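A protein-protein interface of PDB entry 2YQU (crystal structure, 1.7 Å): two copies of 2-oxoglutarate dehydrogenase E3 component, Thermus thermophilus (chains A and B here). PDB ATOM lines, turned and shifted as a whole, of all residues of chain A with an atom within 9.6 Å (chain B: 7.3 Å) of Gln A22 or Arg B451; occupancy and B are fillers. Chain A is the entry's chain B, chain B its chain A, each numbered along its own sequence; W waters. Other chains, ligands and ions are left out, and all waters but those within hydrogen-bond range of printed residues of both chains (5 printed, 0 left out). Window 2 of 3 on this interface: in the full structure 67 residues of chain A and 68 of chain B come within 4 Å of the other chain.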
ATOM      1  N   LEU A   4      28.741 -12.117  29.566  1.00  0.00           N
ATOM      2  CA  LEU A   4      28.965 -12.452  28.167  1.00  0.00           C
ATOM      3  C   LEU A   4      27.759 -12.087  27.302  1.00  0.00           C
ATOM      4  O   LEU A   4      26.627 -12.481  27.599  1.00  0.00           O
ATOM      5  CB  LEU A   4      29.251 -13.950  28.030  1.00  0.00           C
ATOM      6  CG  LEU A   4      29.314 -14.489  26.600  1.00  0.00           C
ATOM      7  CD1 LEU A   4      30.436 -13.841  25.790  1.00  0.00           C
ATOM      8  CD2 LEU A   4      29.455 -16.006  26.633  1.00  0.00           C
ATOM      9  N   TYR A  14      25.135 -20.452  20.221  1.00  0.00           N
ATOM     10  CA  TYR A  14      24.193 -21.038  21.167  1.00  0.00           C
ATOM     11  C   TYR A  14      24.889 -22.046  22.079  1.00  0.00           C
ATOM     12  O   TYR A  14      24.590 -22.122  23.262  1.00  0.00           O
ATOM     13  CB  TYR A  14      22.908 -21.568  20.481  1.00  0.00           C
ATOM     14  CG  TYR A  14      22.879 -23.051  20.129  1.00  0.00           C
ATOM     15  CD1 TYR A  14      22.792 -24.017  21.117  1.00  0.00           C
ATOM     16  CD2 TYR A  14      22.874 -23.470  18.798  1.00  0.00           C
ATOM     17  CE1 TYR A  14      22.760 -25.363  20.795  1.00  0.00           C
ATOM     18  CE2 TYR A  14      22.843 -24.809  18.466  1.00  0.00           C
ATOM     19  CZ  TYR A  14      22.777 -25.753  19.472  1.00  0.00           C
ATOM     20  OH  TYR A  14      22.734 -27.091  19.156  1.00  0.00           O
ATOM     21  N   VAL A  15      25.843 -22.804  21.541  1.00  0.00           N
ATOM     22  CA  VAL A  15      26.600 -23.724  22.376  1.00  0.00           C
ATOM     23  C   VAL A  15      27.513 -22.971  23.345  1.00  0.00           C
ATOM     24  O   VAL A  15      27.601 -23.332  24.526  1.00  0.00           O
ATOM     25  CB  VAL A  15      27.391 -24.732  21.521  1.00  0.00           C
ATOM     26  CG1 VAL A  15      28.358 -25.555  22.380  1.00  0.00           C
ATOM     27  CG2 VAL A  15      26.404 -25.631  20.762  1.00  0.00           C
ATOM     28  N   ALA A  16      28.160 -21.911  22.859  1.00  0.00           N
ATOM     29  CA  ALA A  16      28.994 -21.059  23.711  1.00  0.00           C
ATOM     30  C   ALA A  16      28.164 -20.497  24.864  1.00  0.00           C
ATOM     31  O   ALA A  16      28.621 -20.478  25.997  1.00  0.00           O
ATOM     32  CB  ALA A  16      29.589 -19.930  22.921  1.00  0.00           C
ATOM     33  N   ALA A  17      26.942 -20.055  24.561  1.00  0.00           N
ATOM     34  CA  ALA A  17      26.046 -19.488  25.571  1.00  0.00           C
ATOM     35  C   ALA A  17      25.701 -20.505  26.650  1.00  0.00           C
ATOM     36  O   ALA A  17      25.721 -20.174  27.824  1.00  0.00           O
ATOM     37  CB  ALA A  17      24.765 -18.935  24.930  1.00  0.00           C
ATOM     38  N   ILE A  18      25.411 -21.750  26.254  1.00  0.00           N
ATOM     39  CA  ILE A  18      25.102 -22.806  27.219  1.00  0.00           C
ATOM     40  C   ILE A  18      26.326 -23.123  28.078  1.00  0.00           C
ATOM     41  O   ILE A  18      26.223 -23.173  29.299  1.00  0.00           O
ATOM     42  CB  ILE A  18      24.571 -24.080  26.524  1.00  0.00           C
ATOM     43  CG1 ILE A  18      23.220 -23.807  25.862  1.00  0.00           C
ATOM     44  CG2 ILE A  18      24.421 -25.223  27.528  1.00  0.00           C
ATOM     45  CD1 ILE A  18      22.808 -24.834  24.829  1.00  0.00           C
ATOM     46  N   ARG A  19      27.479 -23.327  27.445  1.00  0.00           N
ATOM     47  CA  ARG A  19      28.703 -23.589  28.195  1.00  0.00           C
ATOM     48  C   ARG A  19      29.034 -22.457  29.174  1.00  0.00           C
ATOM     49  O   ARG A  19      29.425 -22.715  30.312  1.00  0.00           O
ATOM     50  CB  ARG A  19      29.887 -23.836  27.263  1.00  0.00           C
ATOM     51  CG  ARG A  19      31.139 -24.287  27.998  1.00  0.00           C
ATOM     52  CD  ARG A  19      31.017 -25.667  28.655  1.00  0.00           C
ATOM     53  NE  ARG A  19      32.198 -25.959  29.462  1.00  0.00           N
ATOM     54  CZ  ARG A  19      32.194 -26.514  30.671  1.00  0.00           C
ATOM     55  NH1 ARG A  19      31.068 -26.844  31.286  1.00  0.00           N
ATOM     56  NH2 ARG A  19      33.345 -26.724  31.285  1.00  0.00           N
ATOM     57  N   ALA A  20      28.871 -21.218  28.722  1.00  0.00           N
ATOM     58  CA  ALA A  20      29.120 -20.040  29.543  1.00  0.00           C
ATOM     59  C   ALA A  20      28.227 -20.027  30.786  1.00  0.00           C
ATOM     60  O   ALA A  20      28.695 -19.767  31.892  1.00  0.00           O
ATOM     61  CB  ALA A  20      28.896 -18.787  28.728  1.00  0.00           C
ATOM     62  N   ALA A  21      26.942 -20.308  30.596  1.00  0.00           N
ATOM     63  CA  ALA A  21      26.007 -20.399  31.718  1.00  0.00           C
ATOM     64  C   ALA A  21      26.411 -21.507  32.686  1.00  0.00           C
ATOM     65  O   ALA A  21      26.328 -21.337  33.901  1.00  0.00           O
ATOM     66  CB  ALA A  21      24.577 -20.608  31.218  1.00  0.00           C
ATOM     67  N   GLN A  22      26.862 -22.637  32.144  1.00  0.00           N
ATOM     68  CA  GLN A  22      27.361 -23.740  32.962  1.00  0.00           C
ATOM     69  C   GLN A  22      28.562 -23.333  33.813  1.00  0.00           C
ATOM     70  O   GLN A  22      28.738 -23.860  34.909  1.00  0.00           O
ATOM     71  CB  GLN A  22      27.738 -24.942  32.084  1.00  0.00           C
ATOM     72  CG  GLN A  22      26.545 -25.678  31.500  1.00  0.00           C
ATOM     73  CD  GLN A  22      26.953 -26.886  30.667  1.00  0.00           C
ATOM     74  OE1 GLN A  22      28.134 -27.071  30.373  1.00  0.00           O
ATOM     75  NE2 GLN A  22      25.981 -27.702  30.286  1.00  0.00           N
ATOM     76  N   LEU A  23      29.362 -22.391  33.310  1.00  0.00           N
ATOM     77  CA  LEU A  23      30.564 -21.895  33.992  1.00  0.00           C
ATOM     78  C   LEU A  23      30.240 -20.735  34.941  1.00  0.00           C
ATOM     79  O   LEU A  23      31.124 -20.203  35.598  1.00  0.00           O
ATOM     80  CB  LEU A  23      31.614 -21.450  32.964  1.00  0.00           C
ATOM     81  CG  LEU A  23      32.302 -22.554  32.151  1.00  0.00           C
ATOM     82  CD1 LEU A  23      33.111 -21.955  31.015  1.00  0.00           C
ATOM     83  CD2 LEU A  23      33.189 -23.404  33.055  1.00  0.00           C
ATOM     84  N   GLY A  24      28.969 -20.351  34.980  1.00  0.00           N
ATOM     85  CA  GLY A  24      28.461 -19.386  35.937  1.00  0.00           C
ATOM     86  C   GLY A  24      28.392 -17.964  35.416  1.00  0.00           C
ATOM     87  O   GLY A  24      28.237 -17.033  36.204  1.00  0.00           O
ATOM     88  N   MET A  25      28.516 -17.777  34.105  1.00  0.00           N
ATOM     89  CA  MET A  25      28.399 -16.441  33.522  1.00  0.00           C
ATOM     90  C   MET A  25      26.939 -16.054  33.357  1.00  0.00           C
ATOM     91  O   MET A  25      26.086 -16.900  33.139  1.00  0.00           O
ATOM     92  CB  MET A  25      29.071 -16.377  32.147  1.00  0.00           C
ATOM     93  CG  MET A  25      30.547 -16.668  32.169  1.00  0.00           C
ATOM     94  SD  MET A  25      31.280 -16.499  30.540  1.00  0.00           S
ATOM     95  CE  MET A  25      31.874 -14.852  30.631  1.00  0.00           C
ATOM     96  N   LYS A  26      26.670 -14.757  33.465  1.00  0.00           N
ATOM     97  CA  LYS A  26      25.389 -14.192  33.092  1.00  0.00           C
ATOM     98  C   LYS A  26      25.442 -13.874  31.608  1.00  0.00           C
ATOM     99  O   LYS A  26      26.247 -13.057  31.179  1.00  0.00           O
ATOM    100  CB  LYS A  26      25.099 -12.919  33.891  1.00  0.00           C
ATOM    101  CG  LYS A  26      23.778 -12.274  33.531  1.00  0.00           C
ATOM    102  CD  LYS A  26      23.600 -10.914  34.198  1.00  0.00           C
ATOM    103  CE  LYS A  26      22.213 -10.363  33.947  1.00  0.00           C
ATOM    104  NZ  LYS A  26      22.171  -8.882  34.011  1.00  0.00           N
ATOM    105  N   VAL A  27      24.572 -14.514  30.831  1.00  0.00           N
ATOM    106  CA  VAL A  27      24.693 -14.515  29.377  1.00  0.00           C
ATOM    107  C   VAL A  27      23.466 -13.913  28.698  1.00  0.00           C
ATOM    108  O   VAL A  27      22.332 -14.219  29.063  1.00  0.00           O
ATOM    109  CB  VAL A  27      24.895 -15.957  28.833  1.00  0.00           C
ATOM    110  CG1 VAL A  27      25.154 -15.939  27.320  1.00  0.00           C
ATOM    111  CG2 VAL A  27      26.019 -16.662  29.574  1.00  0.00           C
ATOM    112  N   LEU A  98      16.696 -25.121  25.935  1.00  0.00           N
ATOM    113  CA  LEU A  98      17.989 -25.095  26.610  1.00  0.00           C
ATOM    114  C   LEU A  98      18.389 -23.691  27.078  1.00  0.00           C
ATOM    115  O   LEU A  98      19.053 -23.560  28.102  1.00  0.00           O
ATOM    116  CB  LEU A  98      19.083 -25.695  25.719  1.00  0.00           C
ATOM    117  CG  LEU A  98      18.924 -27.191  25.425  1.00  0.00           C
ATOM    118  CD1 LEU A  98      19.781 -27.568  24.232  1.00  0.00           C
ATOM    119  CD2 LEU A  98      19.298 -28.008  26.636  1.00  0.00           C
ATOM    120  N   LYS A 101      16.305 -23.134  30.130  1.00  0.00           N
ATOM    121  CA  LYS A 101      16.808 -23.985  31.204  1.00  0.00           C
ATOM    122  C   LYS A 101      18.061 -23.393  31.840  1.00  0.00           C
ATOM    123  O   LYS A 101      18.216 -23.412  33.062  1.00  0.00           O
ATOM    124  CB  LYS A 101      17.103 -25.400  30.708  1.00  0.00           C
ATOM    125  CG  LYS A 101      17.838 -26.243  31.754  1.00  0.00           C
ATOM    126  CD  LYS A 101      17.809 -27.727  31.462  1.00  0.00           C
ATOM    127  CE  LYS A 101      18.918 -28.434  32.244  1.00  0.00           C
ATOM    128  NZ  LYS A 101      18.821 -29.917  32.174  1.00  0.00           N
ATOM    129  N   ASN A 102      18.942 -22.858  31.005  1.00  0.00           N
ATOM    130  CA  ASN A 102      20.236 -22.362  31.461  1.00  0.00           C
ATOM    131  C   ASN A 102      20.232 -20.876  31.857  1.00  0.00           C
ATOM    132  O   ASN A 102      21.283 -20.320  32.208  1.00  0.00           O
ATOM    133  CB  ASN A 102      21.295 -22.619  30.386  1.00  0.00           C
ATOM    134  CG  ASN A 102      21.730 -24.079  30.340  1.00  0.00           C
ATOM    135  OD1 ASN A 102      22.491 -24.536  31.198  1.00  0.00           O
ATOM    136  ND2 ASN A 102      21.239 -24.815  29.356  1.00  0.00           N
ATOM    137  N   GLY A 103      19.071 -20.231  31.782  1.00  0.00           N
ATOM    138  CA  GLY A 103      18.939 -18.839  32.197  1.00  0.00           C
ATOM    139  C   GLY A 103      19.596 -17.829  31.272  1.00  0.00           C
ATOM    140  O   GLY A 103      19.990 -16.737  31.694  1.00  0.00           O
ATOM    141  N   ILE A 104      19.716 -18.202  30.004  1.00  0.00           N
ATOM    142  CA  ILE A 104      20.259 -17.336  28.966  1.00  0.00           C
ATOM    143  C   ILE A 104      19.177 -16.402  28.438  1.00  0.00           C
ATOM    144  O   ILE A 104      18.101 -16.837  28.009  1.00  0.00           O
ATOM    145  CB  ILE A 104      20.835 -18.192  27.827  1.00  0.00           C
ATOM    146  CG1 ILE A 104      22.007 -19.028  28.348  1.00  0.00           C
ATOM    147  CG2 ILE A 104      21.289 -17.316  26.658  1.00  0.00           C
ATOM    148  CD1 ILE A 104      22.267 -20.294  27.550  1.00  0.00           C
ATOM    149  N   ILE A 318      32.984 -23.420  22.780  1.00  0.00           N
ATOM    150  CA  ILE A 318      33.322 -23.969  24.088  1.00  0.00           C
ATOM    151  C   ILE A 318      34.689 -23.440  24.527  1.00  0.00           C
ATOM    152  O   ILE A 318      34.858 -23.022  25.684  1.00  0.00           O
ATOM    153  CB  ILE A 318      33.289 -25.527  24.073  1.00  0.00           C
ATOM    154  CG1 ILE A 318      31.836 -26.005  23.953  1.00  0.00           C
ATOM    155  CG2 ILE A 318      33.920 -26.090  25.342  1.00  0.00           C
ATOM    156  CD1 ILE A 318      31.686 -27.414  23.461  1.00  0.00           C
ATOM    157  N   VAL A 321      34.764 -19.591  25.631  1.00  0.00           N
ATOM    158  CA  VAL A 321      34.184 -19.288  26.935  1.00  0.00           C
ATOM    159  C   VAL A 321      34.978 -19.917  28.074  1.00  0.00           C
ATOM    160  O   VAL A 321      35.023 -19.376  29.168  1.00  0.00           O
ATOM    161  CB  VAL A 321      32.672 -19.631  27.002  1.00  0.00           C
ATOM    162  CG1 VAL A 321      31.927 -18.891  25.907  1.00  0.00           C
ATOM    163  CG2 VAL A 321      32.416 -21.110  26.908  1.00  0.00           C
ATOM    164  N   GLU A 322      35.623 -21.050  27.812  1.00  0.00           N
ATOM    165  CA  GLU A 322      36.510 -21.658  28.796  1.00  0.00           C
ATOM    166  C   GLU A 322      37.767 -20.808  28.974  1.00  0.00           C
ATOM    167  O   GLU A 322      38.323 -20.763  30.069  1.00  0.00           O
ATOM    168  CB  GLU A 322      36.837 -23.112  28.422  1.00  0.00           C
ATOM    169  CG  GLU A 322      35.637 -24.023  28.667  1.00  0.00           C
ATOM    170  CD  GLU A 322      35.874 -25.489  28.353  1.00  0.00           C
ATOM    171  OE1 GLU A 322      34.995 -26.311  28.689  1.00  0.00           O
ATOM    172  OE2 GLU A 322      36.916 -25.826  27.773  1.00  0.00           O
ATOM    173  N   VAL A 325      36.642 -17.656  31.231  1.00  0.00           N
ATOM    174  CA  VAL A 325      36.396 -17.954  32.631  1.00  0.00           C
ATOM    175  C   VAL A 325      37.645 -18.492  33.321  1.00  0.00           C
ATOM    176  O   VAL A 325      37.993 -18.038  34.406  1.00  0.00           O
ATOM    177  CB  VAL A 325      35.228 -18.951  32.772  1.00  0.00           C
ATOM    178  CG1 VAL A 325      35.016 -19.365  34.227  1.00  0.00           C
ATOM    179  CG2 VAL A 325      33.948 -18.332  32.195  1.00  0.00           C
ATOM    180  N   ARG A 326      38.315 -19.446  32.679  1.00  0.00           N
ATOM    181  CA  ARG A 326      39.422 -20.180  33.290  1.00  0.00           C
ATOM    182  C   ARG A 326      40.800 -19.862  32.711  1.00  0.00           C
ATOM    183  O   ARG A 326      41.821 -20.211  33.311  1.00  0.00           O
ATOM    184  CB  ARG A 326      39.166 -21.681  33.160  1.00  0.00           C
ATOM    185  CG  ARG A 326      37.899 -22.141  33.838  1.00  0.00           C
ATOM    186  CD  ARG A 326      37.501 -23.562  33.520  1.00  0.00           C
ATOM    187  NE  ARG A 326      36.585 -24.077  34.536  1.00  0.00           N
ATOM    188  CZ  ARG A 326      35.828 -25.162  34.401  1.00  0.00           C
ATOM    189  NH1 ARG A 326      35.867 -25.894  33.293  1.00  0.00           N
ATOM    190  NH2 ARG A 326      35.032 -25.522  35.401  1.00  0.00           N
ATOM    191  N   GLU B 443      27.367 -36.702  23.996  1.00  0.00           N
ATOM    192  CA  GLU B 443      26.569 -36.065  25.039  1.00  0.00           C
ATOM    193  C   GLU B 443      26.374 -36.997  26.230  1.00  0.00           C
ATOM    194  O   GLU B 443      26.394 -36.547  27.369  1.00  0.00           O
ATOM    195  CB  GLU B 443      25.217 -35.577  24.491  1.00  0.00           C
ATOM    196  CG  GLU B 443      25.296 -34.484  23.431  1.00  0.00           C
ATOM    197  CD  GLU B 443      25.559 -33.087  23.979  1.00  0.00           C
ATOM    198  OE1 GLU B 443      25.340 -32.848  25.179  1.00  0.00           O
ATOM    199  OE2 GLU B 443      26.002 -32.216  23.201  1.00  0.00           O
ATOM    200  N   ALA B 445      28.542 -39.140  27.222  1.00  0.00           N
ATOM    201  CA  ALA B 445      29.837 -39.129  27.888  1.00  0.00           C
ATOM    202  C   ALA B 445      29.994 -37.875  28.731  1.00  0.00           C
ATOM    203  O   ALA B 445      30.449 -37.960  29.857  1.00  0.00           O
ATOM    204  CB  ALA B 445      30.959 -39.231  26.890  1.00  0.00           C
ATOM    205  N   LEU B 446      29.629 -36.722  28.171  1.00  0.00           N
ATOM    206  CA  LEU B 446      29.640 -35.458  28.908  1.00  0.00           C
ATOM    207  C   LEU B 446      28.755 -35.515  30.141  1.00  0.00           C
ATOM    208  O   LEU B 446      29.115 -34.990  31.187  1.00  0.00           O
ATOM    209  CB  LEU B 446      29.154 -34.300  28.033  1.00  0.00           C
ATOM    210  CG  LEU B 446      30.116 -33.787  26.960  1.00  0.00           C
ATOM    211  CD1 LEU B 446      29.423 -32.748  26.111  1.00  0.00           C
ATOM    212  CD2 LEU B 446      31.391 -33.218  27.572  1.00  0.00           C
ATOM    213  N   ALA B 447      27.579 -36.117  29.989  1.00  0.00           N
ATOM    214  CA  ALA B 447      26.626 -36.277  31.084  1.00  0.00           C
ATOM    215  C   ALA B 447      27.178 -37.144  32.210  1.00  0.00           C
ATOM    216  O   ALA B 447      26.866 -36.922  33.372  1.00  0.00           O
ATOM    217  CB  ALA B 447      25.302 -36.858  30.562  1.00  0.00           C
ATOM    218  N   ALA B 448      27.982 -38.145  31.862  1.00  0.00           N
ATOM    219  CA  ALA B 448      28.609 -39.005  32.859  1.00  0.00           C
ATOM    220  C   ALA B 448      29.722 -38.237  33.565  1.00  0.00           C
ATOM    221  O   ALA B 448      29.881 -38.337  34.779  1.00  0.00           O
ATOM    222  CB  ALA B 448      29.165 -40.281  32.198  1.00  0.00           C
ATOM    223  N   TRP B 449      30.473 -37.454  32.795  1.00  0.00           N
ATOM    224  CA  TRP B 449      31.584 -36.670  33.326  1.00  0.00           C
ATOM    225  C   TRP B 449      31.068 -35.629  34.312  1.00  0.00           C
ATOM    226  O   TRP B 449      31.460 -35.601  35.476  1.00  0.00           O
ATOM    227  CB  TRP B 449      32.320 -35.967  32.183  1.00  0.00           C
ATOM    228  CG  TRP B 449      33.244 -34.873  32.631  1.00  0.00           C
ATOM    229  CD1 TRP B 449      34.127 -34.926  33.665  1.00  0.00           C
ATOM    230  CD2 TRP B 449      33.385 -33.567  32.052  1.00  0.00           C
ATOM    231  NE1 TRP B 449      34.813 -33.740  33.767  1.00  0.00           N
ATOM    232  CE2 TRP B 449      34.375 -32.884  32.794  1.00  0.00           C
ATOM    233  CE3 TRP B 449      32.776 -32.900  30.983  1.00  0.00           C
ATOM    234  CZ2 TRP B 449      34.774 -31.571  32.499  1.00  0.00           C
ATOM    235  CZ3 TRP B 449      33.171 -31.583  30.691  1.00  0.00           C
ATOM    236  CH2 TRP B 449      34.161 -30.941  31.449  1.00  0.00           C
ATOM    237  N   GLU B 450      30.177 -34.787  33.817  1.00  0.00           N
ATOM    238  CA  GLU B 450      29.629 -33.682  34.591  1.00  0.00           C
ATOM    239  C   GLU B 450      28.199 -33.435  34.116  1.00  0.00           C
ATOM    240  O   GLU B 450      27.237 -33.905  34.722  1.00  0.00           O
ATOM    241  CB  GLU B 450      30.490 -32.436  34.399  1.00  0.00           C
ATOM    242  CG  GLU B 450      31.737 -32.364  35.263  1.00  0.00           C
ATOM    243  CD  GLU B 450      32.463 -31.028  35.149  1.00  0.00           C
ATOM    244  OE1 GLU B 450      32.275 -30.305  34.144  1.00  0.00           O
ATOM    245  OE2 GLU B 450      33.237 -30.695  36.073  1.00  0.00           O
ATOM    246  N   ARG B 451      28.069 -32.709  33.017  1.00  0.00           N
ATOM    247  CA  ARG B 451      26.767 -32.421  32.429  1.00  0.00           C
ATOM    248  C   ARG B 451      26.908 -32.219  30.926  1.00  0.00           C
ATOM    249  O   ARG B 451      27.917 -31.680  30.462  1.00  0.00           O
ATOM    250  CB  ARG B 451      26.157 -31.164  33.060  1.00  0.00           C
ATOM    251  CG  ARG B 451      27.057 -29.950  32.994  1.00  0.00           C
ATOM    252  CD  ARG B 451      26.486 -28.704  33.665  1.00  0.00           C
ATOM    253  NE  ARG B 451      26.504 -28.829  35.119  1.00  0.00           N
ATOM    254  CZ  ARG B 451      25.486 -29.254  35.868  1.00  0.00           C
ATOM    255  NH1 ARG B 451      24.328 -29.607  35.320  1.00  0.00           N
ATOM    256  NH2 ARG B 451      25.630 -29.328  37.188  1.00  0.00           N
ATOM    257  N   PRO B 452      25.883 -32.611  30.174  1.00  0.00           N
ATOM    258  CA  PRO B 452      25.881 -32.429  28.724  1.00  0.00           C
ATOM    259  C   PRO B 452      25.527 -30.995  28.374  1.00  0.00           C
ATOM    260  O   PRO B 452      25.122 -30.238  29.255  1.00  0.00           O
ATOM    261  CB  PRO B 452      24.765 -33.366  28.263  1.00  0.00           C
ATOM    262  CG  PRO B 452      23.809 -33.380  29.385  1.00  0.00           C
ATOM    263  CD  PRO B 452      24.620 -33.214  30.641  1.00  0.00           C
ATOM    264  N   ILE B 453      25.675 -30.645  27.106  1.00  0.00           N
ATOM    265  CA  ILE B 453      25.228 -29.354  26.606  1.00  0.00           C
ATOM    266  C   ILE B 453      23.736 -29.392  26.246  1.00  0.00           C
ATOM    267  O   ILE B 453      23.008 -28.428  26.503  1.00  0.00           O
ATOM    268  CB  ILE B 453      26.088 -28.932  25.386  1.00  0.00           C
ATOM    269  CG1 ILE B 453      27.535 -28.645  25.828  1.00  0.00           C
ATOM    270  CG2 ILE B 453      25.481 -27.727  24.670  1.00  0.00           C
ATOM    271  CD1 ILE B 453      27.730 -27.327  26.563  1.00  0.00           C
ATOM    272  N   HIS B 454      23.279 -30.504  25.680  1.00  0.00           N
ATOM    273  CA  HIS B 454      21.968 -30.563  25.035  1.00  0.00           C
ATOM    274  C   HIS B 454      20.864 -31.260  25.833  1.00  0.00           C
ATOM    275  O   HIS B 454      19.865 -31.682  25.260  1.00  0.00           O
ATOM    276  CB  HIS B 454      22.108 -31.184  23.644  1.00  0.00           C
ATOM    277  CG  HIS B 454      22.818 -30.298  22.674  1.00  0.00           C
ATOM    278  ND1 HIS B 454      24.183 -30.336  22.493  1.00  0.00           N
ATOM    279  CD2 HIS B 454      22.356 -29.313  21.866  1.00  0.00           C
ATOM    280  CE1 HIS B 454      24.530 -29.432  21.595  1.00  0.00           C
ATOM    281  NE2 HIS B 454      23.440 -28.803  21.196  1.00  0.00           N
ATOM    282  N   LEU B 455      21.028 -31.349  27.150  1.00  0.00           N
ATOM    283  CA  LEU B 455      19.932 -31.749  28.034  1.00  0.00           C
ATOM    284  C   LEU B 455      19.705 -30.712  29.114  1.00  0.00           C
ATOM    285  O   LEU B 455      20.622 -29.976  29.487  1.00  0.00           O
ATOM    286  CB  LEU B 455      20.203 -33.102  28.692  1.00  0.00           C
ATOM    287  CG  LEU B 455      20.029 -34.344  27.820  1.00  0.00           C
ATOM    288  CD1 LEU B 455      20.441 -35.566  28.614  1.00  0.00           C
ATOM    289  CD2 LEU B 455      18.596 -34.480  27.323  1.00  0.00           C
ATOM    290  OXT LEU B 455      18.588 -30.666  29.612  1.00  0.00           O
HETATM  291  O   HOH W   1      33.197 -27.942  34.158  1.00  0.00           O
HETATM  292  O   HOH W   2      27.290 -25.961  35.706  1.00  0.00           O
HETATM  293  O   HOH W   3      29.164 -29.560  29.218  1.00  0.00           O
HETATM  294  O   HOH W   4      22.001 -27.633  28.955  1.00  0.00           O
HETATM  295  O   HOH W   5      30.127 -29.651  32.310  1.00  0.00           O
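NE2 of Gln A22 lies within hydrogen-bond range of O of Pro B452, 2.9 Å away. NE2 of His B454 lies within hydrogen-bond range of OH of Tyr A14 (2.8 Å). The side-chain amino group (NZ) of Lys A101 lies within salt-bridge range of the chain-end carboxylate (OXT) of Leu B455 (2.7 Å).
The backbone NH (N) of Ile B453 sits at hydrogen-bond distance from the side-chain carboxylate (OE1) of Glu B443 (2.9 Å). The backbone carbonyl oxygen (O) of Leu B446 lies within hydrogen-bond range of the backbone NH (N) of Arg B451 (3.1 Å). The side-chain carboxylate (OE2) of Glu B443 is in hydrogen-bond range of a ring nitrogen (ND1) of His B454. The backbone carbonyl oxygen of Leu A98 lies within hydrogen-bond range of the side-chain amide nitrogen of Asn A102. The guanidinium group (NH1) of Arg A19 sits at hydrogen-bond distance from the side-chain amide oxygen (OE1) of Gln A22 (3.1 Å).
Among the printed residues, merely in contact across the chains: Ile A18 with Ile B453, Gln A22 with Arg B451, Gln A22 with Ile B453, Leu A98 with Ile B453, Leu A98 with His B454 and Leu A98 with Leu B455.
Of chain B, only Arg B451 (3.5 Å), Pro B452 (2.9 Å) and Ile B453 (3.8 Å) come within 4 Å of Gln A22. Arg B451 touches just one residue of chain A: Gln A22. No residue of chain B comes within 4 Å of Ala A21. No residue of chain A comes within 4 Å of Ala B447. Of chain A, only Gln A22 (2.9 Å) comes within 4 Å of Pro B452. Of the printed residues of chain B, Leu A98 touches Ile B453 (3.7 Å), His B454 (3.7 Å) and Leu B455 (3.7 Å). Of the printed residues of chain B, Ile A18 touches Ile B453 (3.6 Å). Printed residues of chain A within 4 Å of Ile B453: Ile A18 (3.6 Å), Gln A22 (3.8 Å) and Leu A98 (3.7 Å). Asn A102 touches none of the printed residues of chain B. The nearest residue of chain B that does not touch Gln A22 is Leu B455 (5.9 Å). The nearest residue of chain A that does not touch Arg B451 is Arg A19 (5.4 Å).
Of the 12 printed residues of chain B, 5 touch a printed residue of chain A. Among the printed residues, 9 pairs touch across the chains.
No position is printed for both chains. Of the 9 pairs that touch across the chains among the printed residues, none has its exchanged pair printed and touching as well.
Water W1 lies within hydrogen-bond range of OE1 of Glu B450 (2.5 Å), NH2 of Arg A19 (3.1 Å) and NH2 of Arg A326 (3.3 Å). Water W2 bridges O of Gln A22 (2.7 Å) and NE of Arg B451 (3.0 Å). Water W3 bridges the backbone carbonyl oxygen (O) of Arg B451 (2.8 Å) and the side-chain amide oxygen (OE1) of Gln A22 (2.9 Å). Water W4 lies within hydrogen-bond range of O of Ile B453 (2.8 Å), O of Leu B455 (2.8 Å) and ND2 of Asn A102 (2.9 Å). Water W5 bridges OE1 of Glu B450 (2.9 Å) and NH1 of Arg A19 (3.1 Å).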
